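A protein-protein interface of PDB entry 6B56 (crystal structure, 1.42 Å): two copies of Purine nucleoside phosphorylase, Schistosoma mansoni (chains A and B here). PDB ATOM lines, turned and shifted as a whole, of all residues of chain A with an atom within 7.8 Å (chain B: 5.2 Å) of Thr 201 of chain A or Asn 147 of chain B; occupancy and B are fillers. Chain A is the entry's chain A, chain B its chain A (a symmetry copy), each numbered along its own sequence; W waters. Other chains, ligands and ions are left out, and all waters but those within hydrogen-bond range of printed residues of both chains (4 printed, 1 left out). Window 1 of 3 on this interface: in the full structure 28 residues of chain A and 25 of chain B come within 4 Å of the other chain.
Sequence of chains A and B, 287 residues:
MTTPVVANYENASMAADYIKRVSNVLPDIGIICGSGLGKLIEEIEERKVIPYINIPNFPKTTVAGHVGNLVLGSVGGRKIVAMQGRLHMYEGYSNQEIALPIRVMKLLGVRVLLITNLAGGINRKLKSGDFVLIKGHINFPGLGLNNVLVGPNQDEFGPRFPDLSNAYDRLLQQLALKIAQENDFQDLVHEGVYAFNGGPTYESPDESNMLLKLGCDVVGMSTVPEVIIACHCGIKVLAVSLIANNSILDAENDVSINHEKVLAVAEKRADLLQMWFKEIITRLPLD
Of the printed residues of chain B, Gly 198 of chain A touches Gly 142 (3.6 Å) and Leu 145 (3.7 Å). Thr 201 of chain A touches five residues of chain B. Ser 204 of chain A touches none of the printed residues of chain B. Pro 141 of chain B touches none of the printed residues of chain A. Printed residues of chain A within 4 Å of Val 150 of chain B: Tyr 90 (3.4 Å) and Gly 199 (3.6 Å). Printed residues of chain A within 4 Å of Ile 228 of chain B: Thr 201 (3.9 Å). The nearest printed residue of chain A that does not touch Val 150 of chain B is Pro 200 of chain A (4.1 Å).
OG1 of Thr 201 of chain A sits at hydrogen-bond distance from ND2 of Asn 147 of chain B, at 2.9 Å. O of Pro 162 of chain B is in hydrogen-bond range of N of Tyr 202 of chain A, at 3.1 Å. The side-chain amide nitrogen (ND2) of Asn 146 of chain A is in hydrogen-bond range of the side-chain amide oxygen (OD1) of Asn 146 of chain B (3.4 Å). OE2 of Glu 207 of chain A is in hydrogen-bond range of N of Asn 139 of chain B, at 2.9 Å.
Asn 146 of chain A touches its own counterpart, Asn 146 of chain B. 1 position is printed for both chains.
The side-chain amide oxygen (OD1) of Asn 147 of chain B is in hydrogen-bond range of the backbone NH (N) of Leu 149 of chain B (3.0 Å). The backbone NH (N) of Gly 142 of chain B sits at hydrogen-bond distance from the side-chain amide oxygen (OD1) of Asn 139 of chain B. ND2 of Asn 197 of chain A lies within hydrogen-bond range of O of Thr 201 of chain A. The side-chain amide nitrogen (ND2) of Asn 95 of chain B is in hydrogen-bond range of the backbone carbonyl oxygen (O) of Asn 147 of chain B. The backbone carbonyl oxygen (O) of Pro 141 of chain B lies within hydrogen-bond range of the backbone NH (N) of Asn 146 of chain B (2.8 Å). OD1 of Asn 197 of chain A lies close to N of Gly 199 of chain A.
Among the printed residues, merely in contact across the chains: Tyr 90 of chain A with Val 150 of chain B (3.4 Å), Tyr 90 of chain A with Phe 161 of chain B (3.3 Å), Asn 146 of chain A with Leu 145 of chain B (3.7 Å), Asn 197 of chain A with Gly 142 of chain B (3.6 Å), Gly 198 of chain A with Gly 142 of chain B (3.6 Å), Gly 198 of chain A with Leu 145 of chain B (3.7 Å), Gly 199 of chain A with Gly 142 of chain B (3.7 Å), Gly 199 of chain A with Asn 147 of chain B (3.2 Å), Gly 199 of chain A with Val 150 of chain B (3.6 Å), Pro 200 of chain A with Leu 149 of chain B (3.6 Å), Pro 200 of chain A with Phe 161 of chain B (3.4 Å), Pro 200 of chain A with Pro 162 of chain B (3.9 Å), Thr 201 of chain A with Leu 149 of chain B (3.9 Å), Thr 201 of chain A with Pro 162 of chain B (3.6 Å), Thr 201 of chain A with Leu 164 of chain B (3.8 Å), Thr 201 of chain A with Ile 228 of chain B (3.9 Å), Tyr 202 of chain A with Phe 161 of chain B (3.3 Å) and Met 221 of chain A with Phe 161 of chain B (3.97 Å).
Of the 14 printed residues of chain B, 11 touch a printed residue of chain A. Of the 13 printed residues of chain A, 10 touch a printed residue of chain B.
Water W2 lies within hydrogen-bond range of the backbone NH of Leu 164 of chain B (2.8 Å), the backbone carbonyl oxygen of Tyr 202 of chain A (3.0 Å) and the backbone carbonyl oxygen of Glu 203 of chain A (3.1 Å). Water W3 bridges OE2 of Glu 207 of chain A (2.8 Å) and ND2 of Asn 139 of chain B (3.1 Å). Water W4 lies within hydrogen-bond range of OD1 of Asn 197 of chain A (2.9 Å), ND2 of Asn 147 of chain B (3.0 Å), O of Gly 142 of chain B (3.3 Å) and OG1 of Thr 201 of chain A (3.3 Å). Water W1 lies within hydrogen-bond range of OD1 of Asn 146 of chain B (3.1 Å) and OD1 of Asn 146 of chain A (3.1 Å).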
ATOM      1  N   TYR A  90     -24.884  10.896  11.740  1.00  0.00           N
ATOM      2  CA  TYR A  90     -26.215  11.194  11.195  1.00  0.00           C
ATOM      3  C   TYR A  90     -27.239  10.108  11.552  1.00  0.00           C
ATOM      4  O   TYR A  90     -28.447  10.333  11.389  1.00  0.00           O
ATOM      5  CB  TYR A  90     -26.188  11.427   9.671  1.00  0.00           C
ATOM      6  CG  TYR A  90     -25.597  10.287   8.872  1.00  0.00           C
ATOM      7  CD1 TYR A  90     -26.318   9.103   8.650  1.00  0.00           C
ATOM      8  CD2 TYR A  90     -24.314  10.376   8.352  1.00  0.00           C
ATOM      9  CE1 TYR A  90     -25.749   8.044   7.946  1.00  0.00           C
ATOM     10  CE2 TYR A  90     -23.737   9.310   7.664  1.00  0.00           C
ATOM     11  CZ  TYR A  90     -24.465   8.162   7.462  1.00  0.00           C
ATOM     12  OH  TYR A  90     -23.883   7.113   6.785  1.00  0.00           O
ATOM     13  N   ASN A 146     -21.403  20.577  18.659  1.00  0.00           N
ATOM     14  CA  ASN A 146     -21.584  19.134  18.489  1.00  0.00           C
ATOM     15  C   ASN A 146     -20.258  18.395  18.226  1.00  0.00           C
ATOM     16  O   ASN A 146     -20.250  17.325  17.579  1.00  0.00           O
ATOM     17  CB  ASN A 146     -22.623  18.811  17.391  1.00  0.00           C
ATOM     18  CG  ASN A 146     -24.077  18.997  17.862  1.00  0.00           C
ATOM     19  OD1 ASN A 146     -24.369  18.860  19.056  1.00  0.00           O
ATOM     20  ND2 ASN A 146     -24.981  19.335  16.951  1.00  0.00           N
ATOM     21  N   ASN A 197     -19.976  17.857   6.776  1.00  0.00           N
ATOM     22  CA  ASN A 197     -21.425  18.096   6.776  1.00  0.00           C
ATOM     23  C   ASN A 197     -22.066  16.995   7.612  1.00  0.00           C
ATOM     24  O   ASN A 197     -21.987  15.815   7.250  1.00  0.00           O
ATOM     25  CB  ASN A 197     -21.938  18.020   5.331  1.00  0.00           C
ATOM     26  CG  ASN A 197     -23.466  17.905   5.225  1.00  0.00           C
ATOM     27  OD1 ASN A 197     -24.191  18.406   6.080  1.00  0.00           O
ATOM     28  ND2 ASN A 197     -23.946  17.230   4.162  1.00  0.00           N
ATOM     29  N   GLY A 198     -22.677  17.363   8.737  1.00  0.00           N
ATOM     30  CA  GLY A 198     -23.267  16.344   9.602  1.00  0.00           C
ATOM     31  C   GLY A 198     -24.196  15.367   8.888  1.00  0.00           C
ATOM     32  O   GLY A 198     -24.263  14.185   9.253  1.00  0.00           O
ATOM     33  N   GLY A 199     -24.962  15.850   7.915  1.00  0.00           N
ATOM     34  CA  GLY A 199     -25.857  14.996   7.131  1.00  0.00           C
ATOM     35  C   GLY A 199     -27.185  14.673   7.816  1.00  0.00           C
ATOM     36  O   GLY A 199     -27.493  15.236   8.878  1.00  0.00           O
ATOM     37  N   PRO A 200     -28.002  13.769   7.221  1.00  0.00           N
ATOM     38  CA  PRO A 200     -27.731  12.850   6.090  1.00  0.00           C
ATOM     39  C   PRO A 200     -28.125  13.375   4.708  1.00  0.00           C
ATOM     40  O   PRO A 200     -27.968  12.629   3.723  1.00  0.00           O
ATOM     41  CB  PRO A 200     -28.597  11.626   6.439  1.00  0.00           C
ATOM     42  CG  PRO A 200     -29.813  12.242   7.104  1.00  0.00           C
ATOM     43  CD  PRO A 200     -29.271  13.437   7.889  1.00  0.00           C
ATOM     44  N   THR A 201     -28.698  14.583   4.598  1.00  0.00           N
ATOM     45  CA  THR A 201     -28.918  15.155   3.270  1.00  0.00           C
ATOM     46  C   THR A 201     -27.596  15.529   2.612  1.00  0.00           C
ATOM     47  O   THR A 201     -26.701  16.080   3.265  1.00  0.00           O
ATOM     48  CB  THR A 201     -29.815  16.401   3.336  1.00  0.00           C
ATOM     49  OG1 THR A 201     -29.287  17.355   4.271  1.00  0.00           O
ATOM     50  CG2 THR A 201     -31.266  16.037   3.799  1.00  0.00           C
ATOM     51  N   TYR A 202     -27.458  15.224   1.308  1.00  0.00           N
ATOM     52  CA  TYR A 202     -26.327  15.784   0.562  1.00  0.00           C
ATOM     53  C   TYR A 202     -26.329  17.310   0.687  1.00  0.00           C
ATOM     54  O   TYR A 202     -27.386  17.940   0.855  1.00  0.00           O
ATOM     55  CB  TYR A 202     -26.374  15.387  -0.924  1.00  0.00           C
ATOM     56  CG  TYR A 202     -26.162  13.897  -1.138  1.00  0.00           C
ATOM     57  CD1 TYR A 202     -24.903  13.326  -0.964  1.00  0.00           C
ATOM     58  CD2 TYR A 202     -27.219  13.066  -1.475  1.00  0.00           C
ATOM     59  CE1 TYR A 202     -24.707  11.959  -1.143  1.00  0.00           C
ATOM     60  CE2 TYR A 202     -27.019  11.708  -1.664  1.00  0.00           C
ATOM     61  CZ  TYR A 202     -25.773  11.170  -1.473  1.00  0.00           C
ATOM     62  OH  TYR A 202     -25.616   9.800  -1.653  1.00  0.00           O
ATOM     63  N   GLU A 203     -25.138  17.909   0.590  1.00  0.00           N
ATOM     64  CA  GLU A 203     -25.009  19.369   0.548  1.00  0.00           C
ATOM     65  C   GLU A 203     -25.895  19.952  -0.552  1.00  0.00           C
ATOM     66  O   GLU A 203     -25.925  19.447  -1.671  1.00  0.00           O
ATOM     67  CB  GLU A 203     -23.520  19.727   0.297  1.00  0.00           C
ATOM     68  CG  GLU A 203     -22.897  19.281  -1.068  1.00  0.00           C
ATOM     69  CD  GLU A 203     -22.444  17.821  -1.161  1.00  0.00           C
ATOM     70  OE1 GLU A 203     -22.608  17.051  -0.214  1.00  0.00           O
ATOM     71  OE2 GLU A 203     -21.913  17.412  -2.234  1.00  0.00           O
ATOM     72  N   SER A 204     -26.641  21.014  -0.228  1.00  0.00           N
ATOM     73  CA  SER A 204     -27.475  21.678  -1.225  1.00  0.00           C
ATOM     74  C   SER A 204     -26.614  22.447  -2.234  1.00  0.00           C
ATOM     75  O   SER A 204     -25.449  22.750  -1.961  1.00  0.00           O
ATOM     76  CB  SER A 204     -28.440  22.643  -0.547  1.00  0.00           C
ATOM     77  OG  SER A 204     -27.744  23.799  -0.078  1.00  0.00           O
ATOM     78  N   GLU A 207     -25.214  25.454  -0.526  1.00  0.00           N
ATOM     79  CA  GLU A 207     -24.177  25.078   0.439  1.00  0.00           C
ATOM     80  C   GLU A 207     -22.861  24.746  -0.271  1.00  0.00           C
ATOM     81  O   GLU A 207     -21.783  25.130   0.191  1.00  0.00           O
ATOM     82  CB  GLU A 207     -24.673  23.912   1.308  1.00  0.00           C
ATOM     83  CG  GLU A 207     -25.777  24.302   2.296  1.00  0.00           C
ATOM     84  CD  GLU A 207     -26.644  23.138   2.803  1.00  0.00           C
ATOM     85  OE1 GLU A 207     -26.336  21.949   2.527  1.00  0.00           O
ATOM     86  OE2 GLU A 207     -27.663  23.427   3.484  1.00  0.00           O
ATOM     87  N   VAL A 219     -16.306  17.557   0.469  1.00  0.00           N
ATOM     88  CA  VAL A 219     -17.296  17.533   1.549  1.00  0.00           C
ATOM     89  C   VAL A 219     -17.857  16.125   1.751  1.00  0.00           C
ATOM     90  O   VAL A 219     -18.192  15.427   0.784  1.00  0.00           O
ATOM     91  CB  VAL A 219     -18.430  18.562   1.292  1.00  0.00           C
ATOM     92  CG1 VAL A 219     -19.119  18.341  -0.073  1.00  0.00           C
ATOM     93  CG2 VAL A 219     -19.467  18.590   2.466  1.00  0.00           C
ATOM     94  N   MET A 221     -19.737  13.237   5.122  1.00  0.00           N
ATOM     95  CA  MET A 221     -20.547  13.066   6.333  1.00  0.00           C
ATOM     96  C   MET A 221     -19.900  12.151   7.383  1.00  0.00           C
ATOM     97  O   MET A 221     -20.595  11.689   8.312  1.00  0.00           O
ATOM     98  CB  MET A 221     -21.951  12.528   5.978  1.00  0.00           C
ATOM     99  CG  MET A 221     -22.730  13.284   4.943  1.00  0.00           C
ATOM    100  SD  MET A 221     -24.258  12.348   4.544  1.00  0.00           S
ATOM    101  CE  MET A 221     -24.747  13.217   3.055  1.00  0.00           C
ATOM    102  N   ASN B  95     -36.721  16.624  16.413  1.00  0.00           N
ATOM    103  CA  ASN B  95     -36.844  16.233  15.000  1.00  0.00           C
ATOM    104  C   ASN B  95     -38.124  15.446  14.743  1.00  0.00           C
ATOM    105  O   ASN B  95     -38.779  15.621  13.709  1.00  0.00           O
ATOM    106  CB  ASN B  95     -35.650  15.328  14.594  1.00  0.00           C
ATOM    107  CG  ASN B  95     -34.344  16.039  14.503  1.00  0.00           C
ATOM    108  OD1 ASN B  95     -34.240  17.262  14.658  1.00  0.00           O
ATOM    109  ND2 ASN B  95     -33.299  15.251  14.230  1.00  0.00           N
ATOM    110  N   ASN B 139     -28.291  25.605   5.247  1.00  0.00           N
ATOM    111  CA  ASN B 139     -28.862  24.983   6.458  1.00  0.00           C
ATOM    112  C   ASN B 139     -27.767  24.864   7.529  1.00  0.00           C
ATOM    113  O   ASN B 139     -27.124  23.819   7.657  1.00  0.00           O
ATOM    114  CB  ASN B 139     -29.380  23.604   6.050  1.00  0.00           C
ATOM    115  CG  ASN B 139     -30.064  22.832   7.145  1.00  0.00           C
ATOM    116  OD1 ASN B 139     -30.312  23.318   8.259  1.00  0.00           O
ATOM    117  ND2 ASN B 139     -30.401  21.587   6.810  1.00  0.00           N
ATOM    118  N   PRO B 141     -27.942  24.516  10.848  1.00  0.00           N
ATOM    119  CA  PRO B 141     -28.159  23.324  11.704  1.00  0.00           C
ATOM    120  C   PRO B 141     -27.779  22.000  11.035  1.00  0.00           C
ATOM    121  O   PRO B 141     -27.140  21.136  11.671  1.00  0.00           O
ATOM    122  CB  PRO B 141     -29.650  23.442  12.083  1.00  0.00           C
ATOM    123  CG  PRO B 141     -29.922  24.926  12.007  1.00  0.00           C
ATOM    124  CD  PRO B 141     -29.155  25.374  10.804  1.00  0.00           C
ATOM    125  N   GLY B 142     -28.120  21.816   9.761  1.00  0.00           N
ATOM    126  CA  GLY B 142     -27.784  20.571   9.079  1.00  0.00           C
ATOM    127  C   GLY B 142     -26.285  20.350   8.933  1.00  0.00           C
ATOM    128  O   GLY B 142     -25.769  19.242   9.156  1.00  0.00           O
ATOM    129  N   LEU B 145     -24.737  19.022  12.462  1.00  0.00           N
ATOM    130  CA  LEU B 145     -25.219  17.778  13.107  1.00  0.00           C
ATOM    131  C   LEU B 145     -26.579  17.924  13.793  1.00  0.00           C
ATOM    132  O   LEU B 145     -26.985  17.038  14.588  1.00  0.00           O
ATOM    133  CB  LEU B 145     -24.168  17.128  14.032  1.00  0.00           C
ATOM    134  CG  LEU B 145     -23.403  15.941  13.405  1.00  0.00           C
ATOM    135  CD1 LEU B 145     -22.364  15.438  14.416  1.00  0.00           C
ATOM    136  CD2 LEU B 145     -24.318  14.781  12.935  1.00  0.00           C
ATOM    137  N   ASN B 146     -27.348  18.976  13.461  1.00  0.00           N
ATOM    138  CA  ASN B 146     -28.726  19.151  13.923  1.00  0.00           C
ATOM    139  C   ASN B 146     -29.748  19.123  12.770  1.00  0.00           C
ATOM    140  O   ASN B 146     -30.835  19.732  12.876  1.00  0.00           O
ATOM    141  CB  ASN B 146     -28.890  20.430  14.774  1.00  0.00           C
ATOM    142  CG  ASN B 146     -28.365  20.269  16.213  1.00  0.00           C
ATOM    143  OD1 ASN B 146     -28.360  19.157  16.755  1.00  0.00           O
ATOM    144  ND2 ASN B 146     -27.902  21.352  16.824  1.00  0.00           N
ATOM    145  N   ASN B 147     -29.439  18.422  11.665  1.00  0.00           N
ATOM    146  CA  ASN B 147     -30.411  18.225  10.578  1.00  0.00           C
ATOM    147  C   ASN B 147     -31.676  17.546  11.125  1.00  0.00           C
ATOM    148  O   ASN B 147     -31.611  16.667  11.996  1.00  0.00           O
ATOM    149  CB  ASN B 147     -29.773  17.333   9.490  1.00  0.00           C
ATOM    150  CG  ASN B 147     -30.503  17.377   8.129  1.00  0.00           C
ATOM    151  OD1 ASN B 147     -31.663  16.915   7.998  1.00  0.00           O
ATOM    152  ND2 ASN B 147     -29.795  17.830   7.089  1.00  0.00           N
ATOM    153  N   VAL B 148     -32.841  17.917  10.576  1.00  0.00           N
ATOM    154  CA  VAL B 148     -34.136  17.303  10.954  1.00  0.00           C
ATOM    155  C   VAL B 148     -34.186  15.794  10.702  1.00  0.00           C
ATOM    156  O   VAL B 148     -35.022  15.088  11.297  1.00  0.00           O
ATOM    157  CB  VAL B 148     -35.292  18.069  10.235  1.00  0.00           C
ATOM    158  CG1 VAL B 148     -35.292  17.793   8.720  1.00  0.00           C
ATOM    159  CG2 VAL B 148     -36.668  17.772  10.879  1.00  0.00           C
ATOM    160  N   LEU B 149     -33.319  15.271   9.829  1.00  0.00           N
ATOM    161  CA  LEU B 149     -33.268  13.840   9.509  1.00  0.00           C
ATOM    162  C   LEU B 149     -32.248  13.038  10.336  1.00  0.00           C
ATOM    163  O   LEU B 149     -32.101  11.823  10.114  1.00  0.00           O
ATOM    164  CB  LEU B 149     -33.056  13.637   7.994  1.00  0.00           C
ATOM    165  CG  LEU B 149     -34.295  13.903   7.090  1.00  0.00           C
ATOM    166  CD1 LEU B 149     -33.895  13.834   5.627  1.00  0.00           C
ATOM    167  CD2 LEU B 149     -35.430  12.912   7.360  1.00  0.00           C
ATOM    168  N   VAL B 150     -31.503  13.661  11.268  1.00  0.00           N
ATOM    169  CA  VAL B 150     -30.600  12.888  12.133  1.00  0.00           C
ATOM    170  C   VAL B 150     -31.406  11.905  12.973  1.00  0.00           C
ATOM    171  O   VAL B 150     -32.365  12.283  13.656  1.00  0.00           O
ATOM    172  CB  VAL B 150     -29.749  13.816  13.027  1.00  0.00           C
ATOM    173  CG1 VAL B 150     -28.961  13.024  14.073  1.00  0.00           C
ATOM    174  CG2 VAL B 150     -28.773  14.651  12.182  1.00  0.00           C
ATOM    175  N   PHE B 161     -30.217   8.984   2.247  1.00  0.00           N
ATOM    176  CA  PHE B 161     -29.439  10.159   1.826  1.00  0.00           C
ATOM    177  C   PHE B 161     -30.186  10.935   0.738  1.00  0.00           C
ATOM    178  O   PHE B 161     -29.943  10.718  -0.475  1.00  0.00           O
ATOM    179  CB  PHE B 161     -28.045   9.743   1.314  1.00  0.00           C
ATOM    180  CG  PHE B 161     -27.234   8.871   2.277  1.00  0.00           C
ATOM    181  CD1 PHE B 161     -26.698   9.420   3.432  1.00  0.00           C
ATOM    182  CD2 PHE B 161     -26.981   7.525   2.008  1.00  0.00           C
ATOM    183  CE1 PHE B 161     -25.944   8.643   4.309  1.00  0.00           C
ATOM    184  CE2 PHE B 161     -26.234   6.749   2.883  1.00  0.00           C
ATOM    185  CZ  PHE B 161     -25.709   7.316   4.028  1.00  0.00           C
ATOM    186  N   PRO B 162     -31.090  11.846   1.105  1.00  0.00           N
ATOM    187  CA  PRO B 162     -31.834  12.605   0.085  1.00  0.00           C
ATOM    188  C   PRO B 162     -31.024  13.702  -0.594  1.00  0.00           C
ATOM    189  O   PRO B 162     -30.119  14.310  -0.012  1.00  0.00           O
ATOM    190  CB  PRO B 162     -33.006  13.220   0.867  1.00  0.00           C
ATOM    191  CG  PRO B 162     -32.838  12.825   2.252  1.00  0.00           C
ATOM    192  CD  PRO B 162     -31.583  12.113   2.473  1.00  0.00           C
ATOM    193  N   LEU B 164     -31.400  17.427  -2.259  1.00  0.00           N
ATOM    194  CA  LEU B 164     -32.246  18.614  -2.117  1.00  0.00           C
ATOM    195  C   LEU B 164     -32.174  19.557  -3.322  1.00  0.00           C
ATOM    196  O   LEU B 164     -32.715  20.679  -3.251  1.00  0.00           O
ATOM    197  CB  LEU B 164     -31.883  19.383  -0.841  1.00  0.00           C
ATOM    198  CG  LEU B 164     -31.896  18.573   0.444  1.00  0.00           C
ATOM    199  CD1 LEU B 164     -31.398  19.416   1.642  1.00  0.00           C
ATOM    200  CD2 LEU B 164     -33.290  17.997   0.756  1.00  0.00           C
ATOM    201  N   ILE B 228     -37.266  19.931   4.142  1.00  0.00           N
ATOM    202  CA  ILE B 228     -36.471  18.700   4.067  1.00  0.00           C
ATOM    203  C   ILE B 228     -37.361  17.467   4.258  1.00  0.00           C
ATOM    204  O   ILE B 228     -37.235  16.475   3.518  1.00  0.00           O
ATOM    205  CB  ILE B 228     -35.267  18.759   5.042  1.00  0.00           C
ATOM    206  CG1 ILE B 228     -34.253  19.777   4.495  1.00  0.00           C
ATOM    207  CG2 ILE B 228     -34.630  17.381   5.235  1.00  0.00           C
ATOM    208  CD1 ILE B 228     -33.116  20.063   5.420  1.00  0.00           C
HETATM  209  O   HOH W   1     -27.246  17.710  19.201  1.00  0.00           O
HETATM  210  O   HOH W   2     -28.778  18.256  -1.769  1.00  0.00           O
HETATM  211  O   HOH W   3     -29.562  21.396   3.817  1.00  0.00           O
HETATM  212  O   HOH W   4     -27.081  18.840   6.201  1.00  0.00           O
